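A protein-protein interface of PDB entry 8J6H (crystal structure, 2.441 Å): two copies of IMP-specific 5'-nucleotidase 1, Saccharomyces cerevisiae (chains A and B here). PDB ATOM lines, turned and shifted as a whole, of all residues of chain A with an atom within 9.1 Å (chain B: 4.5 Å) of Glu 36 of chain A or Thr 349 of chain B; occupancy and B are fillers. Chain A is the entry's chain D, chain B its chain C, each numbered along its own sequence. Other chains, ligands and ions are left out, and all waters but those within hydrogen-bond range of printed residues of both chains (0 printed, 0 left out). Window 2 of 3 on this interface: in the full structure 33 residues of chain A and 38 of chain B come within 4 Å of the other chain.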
ATOM      1  N   PHE A  28      15.846  14.993   7.914  1.00  0.00           N
ATOM      2  CA  PHE A  28      17.234  14.597   7.697  1.00  0.00           C
ATOM      3  C   PHE A  28      17.414  13.844   6.380  1.00  0.00           C
ATOM      4  O   PHE A  28      18.259  14.203   5.564  1.00  0.00           O
ATOM      5  CB  PHE A  28      17.729  13.739   8.864  1.00  0.00           C
ATOM      6  CG  PHE A  28      19.118  13.199   8.676  1.00  0.00           C
ATOM      7  CD1 PHE A  28      19.328  11.845   8.474  1.00  0.00           C
ATOM      8  CD2 PHE A  28      20.215  14.045   8.701  1.00  0.00           C
ATOM      9  CE1 PHE A  28      20.605  11.344   8.303  1.00  0.00           C
ATOM     10  CE2 PHE A  28      21.495  13.550   8.527  1.00  0.00           C
ATOM     11  CZ  PHE A  28      21.690  12.198   8.326  1.00  0.00           C
ATOM     12  N   VAL A  29      16.612  12.806   6.171  1.00  0.00           N
ATOM     13  CA  VAL A  29      16.755  11.978   4.978  1.00  0.00           C
ATOM     14  C   VAL A  29      16.288  12.692   3.709  1.00  0.00           C
ATOM     15  O   VAL A  29      16.814  12.443   2.625  1.00  0.00           O
ATOM     16  CB  VAL A  29      15.985  10.648   5.120  1.00  0.00           C
ATOM     17  CG1 VAL A  29      16.612   9.790   6.208  1.00  0.00           C
ATOM     18  CG2 VAL A  29      14.521  10.904   5.421  1.00  0.00           C
ATOM     19  N   LEU A  30      15.314  13.586   3.844  1.00  0.00           N
ATOM     20  CA  LEU A  30      14.745  14.265   2.684  1.00  0.00           C
ATOM     21  C   LEU A  30      15.514  15.519   2.281  1.00  0.00           C
ATOM     22  O   LEU A  30      15.406  15.975   1.143  1.00  0.00           O
ATOM     23  CB  LEU A  30      13.282  14.632   2.944  1.00  0.00           C
ATOM     24  CG  LEU A  30      12.234  13.588   2.553  1.00  0.00           C
ATOM     25  CD1 LEU A  30      10.831  14.112   2.818  1.00  0.00           C
ATOM     26  CD2 LEU A  30      12.394  13.195   1.092  1.00  0.00           C
ATOM     27  N   HIS A  31      16.289  16.079   3.203  1.00  0.00           N
ATOM     28  CA  HIS A  31      16.964  17.344   2.932  1.00  0.00           C
ATOM     29  C   HIS A  31      18.479  17.269   3.106  1.00  0.00           C
ATOM     30  O   HIS A  31      19.226  17.780   2.273  1.00  0.00           O
ATOM     31  CB  HIS A  31      16.384  18.445   3.821  1.00  0.00           C
ATOM     32  CG  HIS A  31      14.919  18.674   3.613  1.00  0.00           C
ATOM     33  ND1 HIS A  31      13.988  18.506   4.615  1.00  0.00           N
ATOM     34  CD2 HIS A  31      14.224  19.044   2.512  1.00  0.00           C
ATOM     35  CE1 HIS A  31      12.783  18.770   4.142  1.00  0.00           C
ATOM     36  NE2 HIS A  31      12.898  19.099   2.868  1.00  0.00           N
ATOM     37  N   ALA A  32      18.934  16.636   4.182  1.00  0.00           N
ATOM     38  CA  ALA A  32      20.368  16.494   4.411  1.00  0.00           C
ATOM     39  C   ALA A  32      20.966  15.428   3.496  1.00  0.00           C
ATOM     40  O   ALA A  32      21.849  15.716   2.691  1.00  0.00           O
ATOM     41  CB  ALA A  32      20.649  16.165   5.869  1.00  0.00           C
ATOM     42  N   VAL A  33      20.473  14.199   3.619  1.00  0.00           N
ATOM     43  CA  VAL A  33      21.003  13.073   2.852  1.00  0.00           C
ATOM     44  C   VAL A  33      20.711  13.207   1.358  1.00  0.00           C
ATOM     45  O   VAL A  33      21.431  12.656   0.524  1.00  0.00           O
ATOM     46  CB  VAL A  33      20.429  11.737   3.359  1.00  0.00           C
ATOM     47  CG1 VAL A  33      21.269  10.571   2.858  1.00  0.00           C
ATOM     48  CG2 VAL A  33      20.385  11.733   4.870  1.00  0.00           C
ATOM     49  N   SER A  34      19.660  13.948   1.022  1.00  0.00           N
ATOM     50  CA  SER A  34      19.289  14.155  -0.374  1.00  0.00           C
ATOM     51  C   SER A  34      20.235  15.130  -1.067  1.00  0.00           C
ATOM     52  O   SER A  34      20.180  15.306  -2.283  1.00  0.00           O
ATOM     53  CB  SER A  34      17.852  14.665  -0.478  1.00  0.00           C
ATOM     54  OG  SER A  34      16.937  13.702   0.012  1.00  0.00           O
ATOM     55  N   HIS A  35      21.096  15.767  -0.284  1.00  0.00           N
ATOM     56  CA  HIS A  35      22.078  16.688  -0.832  1.00  0.00           C
ATOM     57  C   HIS A  35      23.467  16.298  -0.350  1.00  0.00           C
ATOM     58  O   HIS A  35      24.386  17.117  -0.308  1.00  0.00           O
ATOM     59  CB  HIS A  35      21.729  18.125  -0.451  1.00  0.00           C
ATOM     60  CG  HIS A  35      20.341  18.522  -0.851  1.00  0.00           C
ATOM     61  ND1 HIS A  35      19.396  18.947   0.055  1.00  0.00           N
ATOM     62  CD2 HIS A  35      19.735  18.531  -2.063  1.00  0.00           C
ATOM     63  CE1 HIS A  35      18.268  19.214  -0.582  1.00  0.00           C
ATOM     64  NE2 HIS A  35      18.448  18.970  -1.867  1.00  0.00           N
ATOM     65  N   GLU A  36      23.598  15.028   0.019  1.00  0.00           N
ATOM     66  CA  GLU A  36      24.898  14.425   0.261  1.00  0.00           C
ATOM     67  C   GLU A  36      25.596  14.253  -1.080  1.00  0.00           C
ATOM     68  O   GLU A  36      25.014  13.715  -2.022  1.00  0.00           O
ATOM     69  CB  GLU A  36      24.751  13.080   0.976  1.00  0.00           C
ATOM     70  CG  GLU A  36      25.872  12.752   1.952  1.00  0.00           C
ATOM     71  CD  GLU A  36      27.152  12.324   1.263  1.00  0.00           C
ATOM     72  OE1 GLU A  36      27.073  11.766   0.148  1.00  0.00           O
ATOM     73  OE2 GLU A  36      28.239  12.538   1.842  1.00  0.00           O
ATOM     74  N   GLY A  37      26.834  14.722  -1.171  1.00  0.00           N
ATOM     75  CA  GLY A  37      27.574  14.660  -2.415  1.00  0.00           C
ATOM     76  C   GLY A  37      27.611  16.004  -3.119  1.00  0.00           C
ATOM     77  O   GLY A  37      28.495  16.257  -3.936  1.00  0.00           O
ATOM     78  N   ASP A  38      26.648  16.867  -2.805  1.00  0.00           N
ATOM     79  CA  ASP A  38      26.620  18.214  -3.366  1.00  0.00           C
ATOM     80  C   ASP A  38      27.805  19.033  -2.860  1.00  0.00           C
ATOM     81  O   ASP A  38      27.838  19.457  -1.703  1.00  0.00           O
ATOM     82  CB  ASP A  38      25.301  18.916  -3.032  1.00  0.00           C
ATOM     83  CG  ASP A  38      24.109  18.289  -3.733  1.00  0.00           C
ATOM     84  OD1 ASP A  38      24.205  17.112  -4.142  1.00  0.00           O
ATOM     85  OD2 ASP A  38      23.079  18.982  -3.887  1.00  0.00           O
ATOM     86  N   TYR A  39      28.773  19.252  -3.744  1.00  0.00           N
ATOM     87  CA  TYR A  39      30.017  19.926  -3.388  1.00  0.00           C
ATOM     88  C   TYR A  39      29.835  21.433  -3.205  1.00  0.00           C
ATOM     89  O   TYR A  39      30.604  22.077  -2.493  1.00  0.00           O
ATOM     90  CB  TYR A  39      31.082  19.671  -4.461  1.00  0.00           C
ATOM     91  CG  TYR A  39      31.487  18.221  -4.625  1.00  0.00           C
ATOM     92  CD1 TYR A  39      32.497  17.669  -3.846  1.00  0.00           C
ATOM     93  CD2 TYR A  39      30.870  17.410  -5.568  1.00  0.00           C
ATOM     94  CE1 TYR A  39      32.874  16.348  -3.993  1.00  0.00           C
ATOM     95  CE2 TYR A  39      31.240  16.082  -5.722  1.00  0.00           C
ATOM     96  CZ  TYR A  39      32.244  15.558  -4.931  1.00  0.00           C
ATOM     97  OH  TYR A  39      32.617  14.242  -5.081  1.00  0.00           O
ATOM     98  N   ASN A  40      28.810  21.985  -3.848  1.00  0.00           N
ATOM     99  CA  ASN A  40      28.635  23.432  -3.930  1.00  0.00           C
ATOM    100  C   ASN A  40      28.109  24.091  -2.660  1.00  0.00           C
ATOM    101  O   ASN A  40      28.877  24.478  -1.775  1.00  0.00           O
ATOM    102  CB  ASN A  40      27.694  23.773  -5.088  1.00  0.00           C
ATOM    103  CG  ASN A  40      28.412  23.853  -6.418  1.00  0.00           C
ATOM    104  OD1 ASN A  40      29.503  23.308  -6.580  1.00  0.00           O
ATOM    105  ND2 ASN A  40      27.800  24.531  -7.381  1.00  0.00           N
ATOM    106  N   ASP A  41      26.789  24.233  -2.593  1.00  0.00           N
ATOM    107  CA  ASP A  41      26.141  25.015  -1.547  1.00  0.00           C
ATOM    108  C   ASP A  41      25.792  24.175  -0.324  1.00  0.00           C
ATOM    109  O   ASP A  41      24.665  23.702  -0.189  1.00  0.00           O
ATOM    110  CB  ASP A  41      24.877  25.676  -2.102  1.00  0.00           C
ATOM    111  CG  ASP A  41      24.617  27.039  -1.494  1.00  0.00           C
ATOM    112  OD1 ASP A  41      24.946  27.232  -0.305  1.00  0.00           O
ATOM    113  OD2 ASP A  41      24.083  27.916  -2.205  1.00  0.00           O
ATOM    114  N   ASP A  42      26.766  23.988   0.560  1.00  0.00           N
ATOM    115  CA  ASP A  42      26.540  23.260   1.801  1.00  0.00           C
ATOM    116  C   ASP A  42      25.840  24.141   2.829  1.00  0.00           C
ATOM    117  O   ASP A  42      25.045  23.657   3.634  1.00  0.00           O
ATOM    118  CB  ASP A  42      27.862  22.741   2.370  1.00  0.00           C
ATOM    119  CG  ASP A  42      28.303  21.439   1.725  1.00  0.00           C
ATOM    120  OD1 ASP A  42      27.440  20.725   1.172  1.00  0.00           O
ATOM    121  OD2 ASP A  42      29.511  21.127   1.779  1.00  0.00           O
ATOM    122  N   THR A  45      21.925  24.231   2.441  1.00  0.00           N
ATOM    123  CA  THR A  45      21.320  22.993   2.916  1.00  0.00           C
ATOM    124  C   THR A  45      21.312  22.937   4.441  1.00  0.00           C
ATOM    125  O   THR A  45      20.303  22.580   5.049  1.00  0.00           O
ATOM    126  CB  THR A  45      22.061  21.758   2.365  1.00  0.00           C
ATOM    127  OG1 THR A  45      21.987  21.755   0.934  1.00  0.00           O
ATOM    128  CG2 THR A  45      21.435  20.478   2.896  1.00  0.00           C
ATOM    129  N   ALA A 128      24.739  20.127  10.101  1.00  0.00           N
ATOM    130  CA  ALA A 128      25.728  20.070   9.031  1.00  0.00           C
ATOM    131  C   ALA A 128      25.962  18.638   8.555  1.00  0.00           C
ATOM    132  O   ALA A 128      26.486  18.417   7.464  1.00  0.00           O
ATOM    133  CB  ALA A 128      27.035  20.692   9.492  1.00  0.00           C
ATOM    134  N   ARG A 129      25.569  17.671   9.377  1.00  0.00           N
ATOM    135  CA  ARG A 129      25.776  16.263   9.055  1.00  0.00           C
ATOM    136  C   ARG A 129      24.830  15.797   7.954  1.00  0.00           C
ATOM    137  O   ARG A 129      23.666  16.194   7.909  1.00  0.00           O
ATOM    138  CB  ARG A 129      25.602  15.393  10.302  1.00  0.00           C
ATOM    139  CG  ARG A 129      26.535  15.761  11.446  1.00  0.00           C
ATOM    140  CD  ARG A 129      26.739  14.588  12.390  1.00  0.00           C
ATOM    141  NE  ARG A 129      25.482  14.119  12.964  1.00  0.00           N
ATOM    142  CZ  ARG A 129      25.027  14.478  14.160  1.00  0.00           C
ATOM    143  NH1 ARG A 129      23.873  13.999  14.603  1.00  0.00           N
ATOM    144  NH2 ARG A 129      25.727  15.314  14.914  1.00  0.00           N
ATOM    145  N   ARG A 130      25.344  14.949   7.069  1.00  0.00           N
ATOM    146  CA  ARG A 130      24.572  14.465   5.931  1.00  0.00           C
ATOM    147  C   ARG A 130      24.450  12.943   5.943  1.00  0.00           C
ATOM    148  O   ARG A 130      23.654  12.371   5.201  1.00  0.00           O
ATOM    149  CB  ARG A 130      25.215  14.922   4.621  1.00  0.00           C
ATOM    150  CG  ARG A 130      25.497  16.413   4.531  1.00  0.00           C
ATOM    151  CD  ARG A 130      24.241  17.202   4.204  1.00  0.00           C
ATOM    152  NE  ARG A 130      24.533  18.610   3.959  1.00  0.00           N
ATOM    153  CZ  ARG A 130      24.262  19.589   4.816  1.00  0.00           C
ATOM    154  NH1 ARG A 130      23.687  19.313   5.979  1.00  0.00           N
ATOM    155  NH2 ARG A 130      24.564  20.843   4.510  1.00  0.00           N
ATOM    156  N   MET A 131      25.246  12.295   6.789  1.00  0.00           N
ATOM    157  CA  MET A 131      25.281  10.837   6.845  1.00  0.00           C
ATOM    158  C   MET A 131      24.800  10.301   8.191  1.00  0.00           C
ATOM    159  O   MET A 131      24.153   9.256   8.256  1.00  0.00           O
ATOM    160  CB  MET A 131      26.696  10.331   6.560  1.00  0.00           C
ATOM    161  CG  MET A 131      27.204  10.670   5.168  1.00  0.00           C
ATOM    162  SD  MET A 131      26.277   9.676   3.771  1.00  0.00           S
ATOM    163  CE  MET A 131      26.775   7.870   4.308  1.00  0.00           C
ATOM    164  N   VAL A 132      25.127  11.019   9.260  1.00  0.00           N
ATOM    165  CA  VAL A 132      24.718  10.619  10.601  1.00  0.00           C
ATOM    166  C   VAL A 132      23.571  11.490  11.098  1.00  0.00           C
ATOM    167  O   VAL A 132      23.719  12.703  11.250  1.00  0.00           O
ATOM    168  CB  VAL A 132      25.892  10.698  11.596  1.00  0.00           C
ATOM    169  CG1 VAL A 132      25.407  10.444  13.013  1.00  0.00           C
ATOM    170  CG2 VAL A 132      26.979   9.706  11.210  1.00  0.00           C
ATOM    171  N   THR B 295      38.303  15.589   0.690  1.00  0.00           N
ATOM    172  CA  THR B 295      37.025  15.282   1.326  1.00  0.00           C
ATOM    173  C   THR B 295      37.054  15.643   2.808  1.00  0.00           C
ATOM    174  O   THR B 295      36.079  16.168   3.348  1.00  0.00           O
ATOM    175  CB  THR B 295      36.663  13.791   1.171  1.00  0.00           C
ATOM    176  OG1 THR B 295      36.655  13.441  -0.218  1.00  0.00           O
ATOM    177  CG2 THR B 295      35.293  13.505   1.767  1.00  0.00           C
ATOM    178  N   LEU B 299      34.632  18.338   4.704  1.00  0.00           N
ATOM    179  CA  LEU B 299      33.919  17.968   5.921  1.00  0.00           C
ATOM    180  C   LEU B 299      34.239  18.937   7.055  1.00  0.00           C
ATOM    181  O   LEU B 299      33.352  19.352   7.797  1.00  0.00           O
ATOM    182  CB  LEU B 299      34.273  16.538   6.333  1.00  0.00           C
ATOM    183  CG  LEU B 299      33.595  15.427   5.532  1.00  0.00           C
ATOM    184  CD1 LEU B 299      34.425  14.153   5.564  1.00  0.00           C
ATOM    185  CD2 LEU B 299      32.194  15.171   6.067  1.00  0.00           C
ATOM    186  N   GLU B 345      30.369  10.573  10.909  1.00  0.00           N
ATOM    187  CA  GLU B 345      30.032  11.283   9.679  1.00  0.00           C
ATOM    188  C   GLU B 345      31.215  11.278   8.719  1.00  0.00           C
ATOM    189  O   GLU B 345      31.056  11.066   7.518  1.00  0.00           O
ATOM    190  CB  GLU B 345      29.610  12.723   9.987  1.00  0.00           C
ATOM    191  CG  GLU B 345      29.500  13.625   8.765  1.00  0.00           C
ATOM    192  CD  GLU B 345      28.131  13.576   8.115  1.00  0.00           C
ATOM    193  OE1 GLU B 345      27.231  12.905   8.667  1.00  0.00           O
ATOM    194  OE2 GLU B 345      27.953  14.210   7.054  1.00  0.00           O
ATOM    195  N   ILE B 346      32.403  11.502   9.270  1.00  0.00           N
ATOM    196  CA  ILE B 346      33.627  11.570   8.482  1.00  0.00           C
ATOM    197  C   ILE B 346      33.964  10.230   7.828  1.00  0.00           C
ATOM    198  O   ILE B 346      34.210  10.170   6.623  1.00  0.00           O
ATOM    199  CB  ILE B 346      34.815  12.030   9.347  1.00  0.00           C
ATOM    200  CG1 ILE B 346      34.654  13.504   9.724  1.00  0.00           C
ATOM    201  CG2 ILE B 346      36.124  11.829   8.611  1.00  0.00           C
ATOM    202  CD1 ILE B 346      35.629  13.977  10.780  1.00  0.00           C
ATOM    203  N   VAL B 347      33.967   9.162   8.620  1.00  0.00           N
ATOM    204  CA  VAL B 347      34.274   7.829   8.107  1.00  0.00           C
ATOM    205  C   VAL B 347      33.274   7.390   7.041  1.00  0.00           C
ATOM    206  O   VAL B 347      33.663   6.914   5.975  1.00  0.00           O
ATOM    207  CB  VAL B 347      34.306   6.780   9.239  1.00  0.00           C
ATOM    208  CG1 VAL B 347      34.093   5.377   8.689  1.00  0.00           C
ATOM    209  CG2 VAL B 347      35.622   6.860   9.980  1.00  0.00           C
ATOM    210  N   LEU B 348      31.989   7.561   7.332  1.00  0.00           N
ATOM    211  CA  LEU B 348      30.937   7.187   6.394  1.00  0.00           C
ATOM    212  C   LEU B 348      31.046   7.966   5.088  1.00  0.00           C
ATOM    213  O   LEU B 348      30.856   7.408   4.007  1.00  0.00           O
ATOM    214  CB  LEU B 348      29.558   7.405   7.021  1.00  0.00           C
ATOM    215  CG  LEU B 348      29.152   6.414   8.113  1.00  0.00           C
ATOM    216  CD1 LEU B 348      27.812   6.803   8.719  1.00  0.00           C
ATOM    217  CD2 LEU B 348      29.105   5.001   7.559  1.00  0.00           C
ATOM    218  N   THR B 349      31.356   9.254   5.191  1.00  0.00           N
ATOM    219  CA  THR B 349      31.511  10.098   4.011  1.00  0.00           C
ATOM    220  C   THR B 349      32.722   9.664   3.190  1.00  0.00           C
ATOM    221  O   THR B 349      32.664   9.613   1.961  1.00  0.00           O
ATOM    222  CB  THR B 349      31.659  11.584   4.392  1.00  0.00           C
ATOM    223  OG1 THR B 349      30.550  11.985   5.204  1.00  0.00           O
ATOM    224  CG2 THR B 349      31.710  12.455   3.145  1.00  0.00           C
ATOM    225  N   LEU B 350      33.814   9.345   3.878  1.00  0.00           N
ATOM    226  CA  LEU B 350      35.031   8.893   3.215  1.00  0.00           C
ATOM    227  C   LEU B 350      34.821   7.569   2.490  1.00  0.00           C
ATOM    228  O   LEU B 350      35.223   7.413   1.337  1.00  0.00           O
ATOM    229  CB  LEU B 350      36.174   8.756   4.224  1.00  0.00           C
ATOM    230  CG  LEU B 350      36.844  10.049   4.689  1.00  0.00           C
ATOM    231  CD1 LEU B 350      37.905   9.752   5.736  1.00  0.00           C
ATOM    232  CD2 LEU B 350      37.446  10.794   3.507  1.00  0.00           C
ATOM    233  N   GLN B 351      34.188   6.618   3.171  1.00  0.00           N
ATOM    234  CA  GLN B 351      33.971   5.291   2.608  1.00  0.00           C
ATOM    235  C   GLN B 351      33.078   5.348   1.371  1.00  0.00           C
ATOM    236  O   GLN B 351      33.358   4.697   0.368  1.00  0.00           O
ATOM    237  CB  GLN B 351      33.358   4.357   3.653  1.00  0.00           C
ATOM    238  CG  GLN B 351      33.357   2.892   3.245  1.00  0.00           C
ATOM    239  CD  GLN B 351      34.729   2.254   3.356  1.00  0.00           C
ATOM    240  OE1 GLN B 351      35.477   2.522   4.297  1.00  0.00           O
ATOM    241  NE2 GLN B 351      35.070   1.408   2.390  1.00  0.00           N
ATOM    242  N   ASN B 352      32.007   6.133   1.447  1.00  0.00           N
ATOM    243  CA  ASN B 352      31.064   6.250   0.339  1.00  0.00           C
ATOM    244  C   ASN B 352      31.654   6.942  -0.886  1.00  0.00           C
ATOM    245  O   ASN B 352      31.461   6.487  -2.013  1.00  0.00           O
ATOM    246  CB  ASN B 352      29.806   6.993   0.790  1.00  0.00           C
ATOM    247  CG  ASN B 352      28.803   6.082   1.470  1.00  0.00           C
ATOM    248  OD1 ASN B 352      27.868   5.590   0.838  1.00  0.00           O
ATOM    249  ND2 ASN B 352      28.996   5.849   2.764  1.00  0.00           N
ATOM    250  N   THR B 353      32.369   8.041  -0.664  1.00  0.00           N
ATOM    251  CA  THR B 353      32.975   8.788  -1.762  1.00  0.00           C
ATOM    252  C   THR B 353      34.056   7.971  -2.464  1.00  0.00           C
ATOM    253  O   THR B 353      34.081   7.888  -3.693  1.00  0.00           O
ATOM    254  CB  THR B 353      33.586  10.118  -1.277  1.00  0.00           C
ATOM    255  OG1 THR B 353      34.429   9.876  -0.143  1.00  0.00           O
ATOM    256  CG2 THR B 353      32.492  11.098  -0.888  1.00  0.00           C
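Of the 11 printed residues of chain B, 4 touch a printed residue of chain A. Printed residues of chain B that touch a printed residue of chain A: Glu 345, Leu 348, Thr 349 and Asn 352. Hydrophobic or aromatic side chains of chain B that line the printed part of chain A: Leu 348. Hydrophobic or aromatic side chains of chain A within 4 Å of the printed part of chain B: Met 131 and Val 132. Along chain A the printed residues that touch a printed residue of chain B span positions 36 to 132. Among the printed residues, no Asp or Glu carboxylate lies within 4 Å of a Lys or Arg side-chain nitrogen of the other chain.
The side-chain carboxylate of Glu 345 of chain B lies within hydrogen-bond range of the backbone NH of Arg 130 of chain A, 2.7 Å away. The backbone NH (N) of Met 131 of chain A is in hydrogen-bond range of the side-chain carboxylate (OE1) of Glu 345 of chain B. The side-chain carboxylate (OE1) of Glu 345 of chain B lies within hydrogen-bond range of the backbone NH (N) of Val 132 of chain A, at 2.9 Å.
The side-chain hydroxyl of Thr 349 of chain B lies within hydrogen-bond range of the backbone carbonyl oxygen of Glu 345 of chain B. O of Leu 348 of chain B sits at hydrogen-bond distance from ND2 of Asn 352 of chain B (2.7 Å). The side-chain hydroxyl of Thr 353 of chain B is in hydrogen-bond range of the backbone carbonyl oxygen of Thr 349 of chain B (2.8 Å). The backbone carbonyl oxygen of Asp 42 of chain A is in hydrogen-bond range of the guanidinium group of Arg 130 of chain A, at 3.0 Å. The backbone carbonyl oxygen (O) of Ala 128 of chain A lies within hydrogen-bond range of the guanidinium group (NH1) of Arg 130 of chain A, at 3.3 Å. The guanidinium group (NE) of Arg 129 of chain A is in hydrogen-bond range of the backbone carbonyl oxygen (O) of Val 132 of chain A (2.8 Å).
Among the printed residues, pairs that only touch across the chains: Glu 36 of chain A with Thr 349 of chain B, Arg 129 of chain A with Glu 345 of chain B, Met 131 of chain A with Leu 348 of chain B, Met 131 of chain A with Thr 349 of chain B, Met 131 of chain A with Asn 352 of chain B and Val 132 of chain A with Leu 348 of chain B.
Glu 36 of chain A touches just one residue of chain B: Thr 349. Printed residues of chain B within 4 Å of Met 131 of chain A: Glu 345 (2.8 Å), Leu 348 (3.9 Å), Thr 349 (3.6 Å) and Asn 352 (3.4 Å). Of the printed residues of chain B, Val 132 of chain A touches Glu 345 and Leu 348. Of chain A, only Glu 36 (3.7 Å) and Met 131 (3.6 Å) come within 4 Å of Thr 349 of chain B. The nearest printed residue of chain B that does not touch Glu 36 of chain A is Thr 353 of chain B (5.3 Å). The nearest printed residue of chain A that does not touch Asn 352 of chain B is Glu 36 of chain A (5.5 Å).
No position is printed for both chains.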
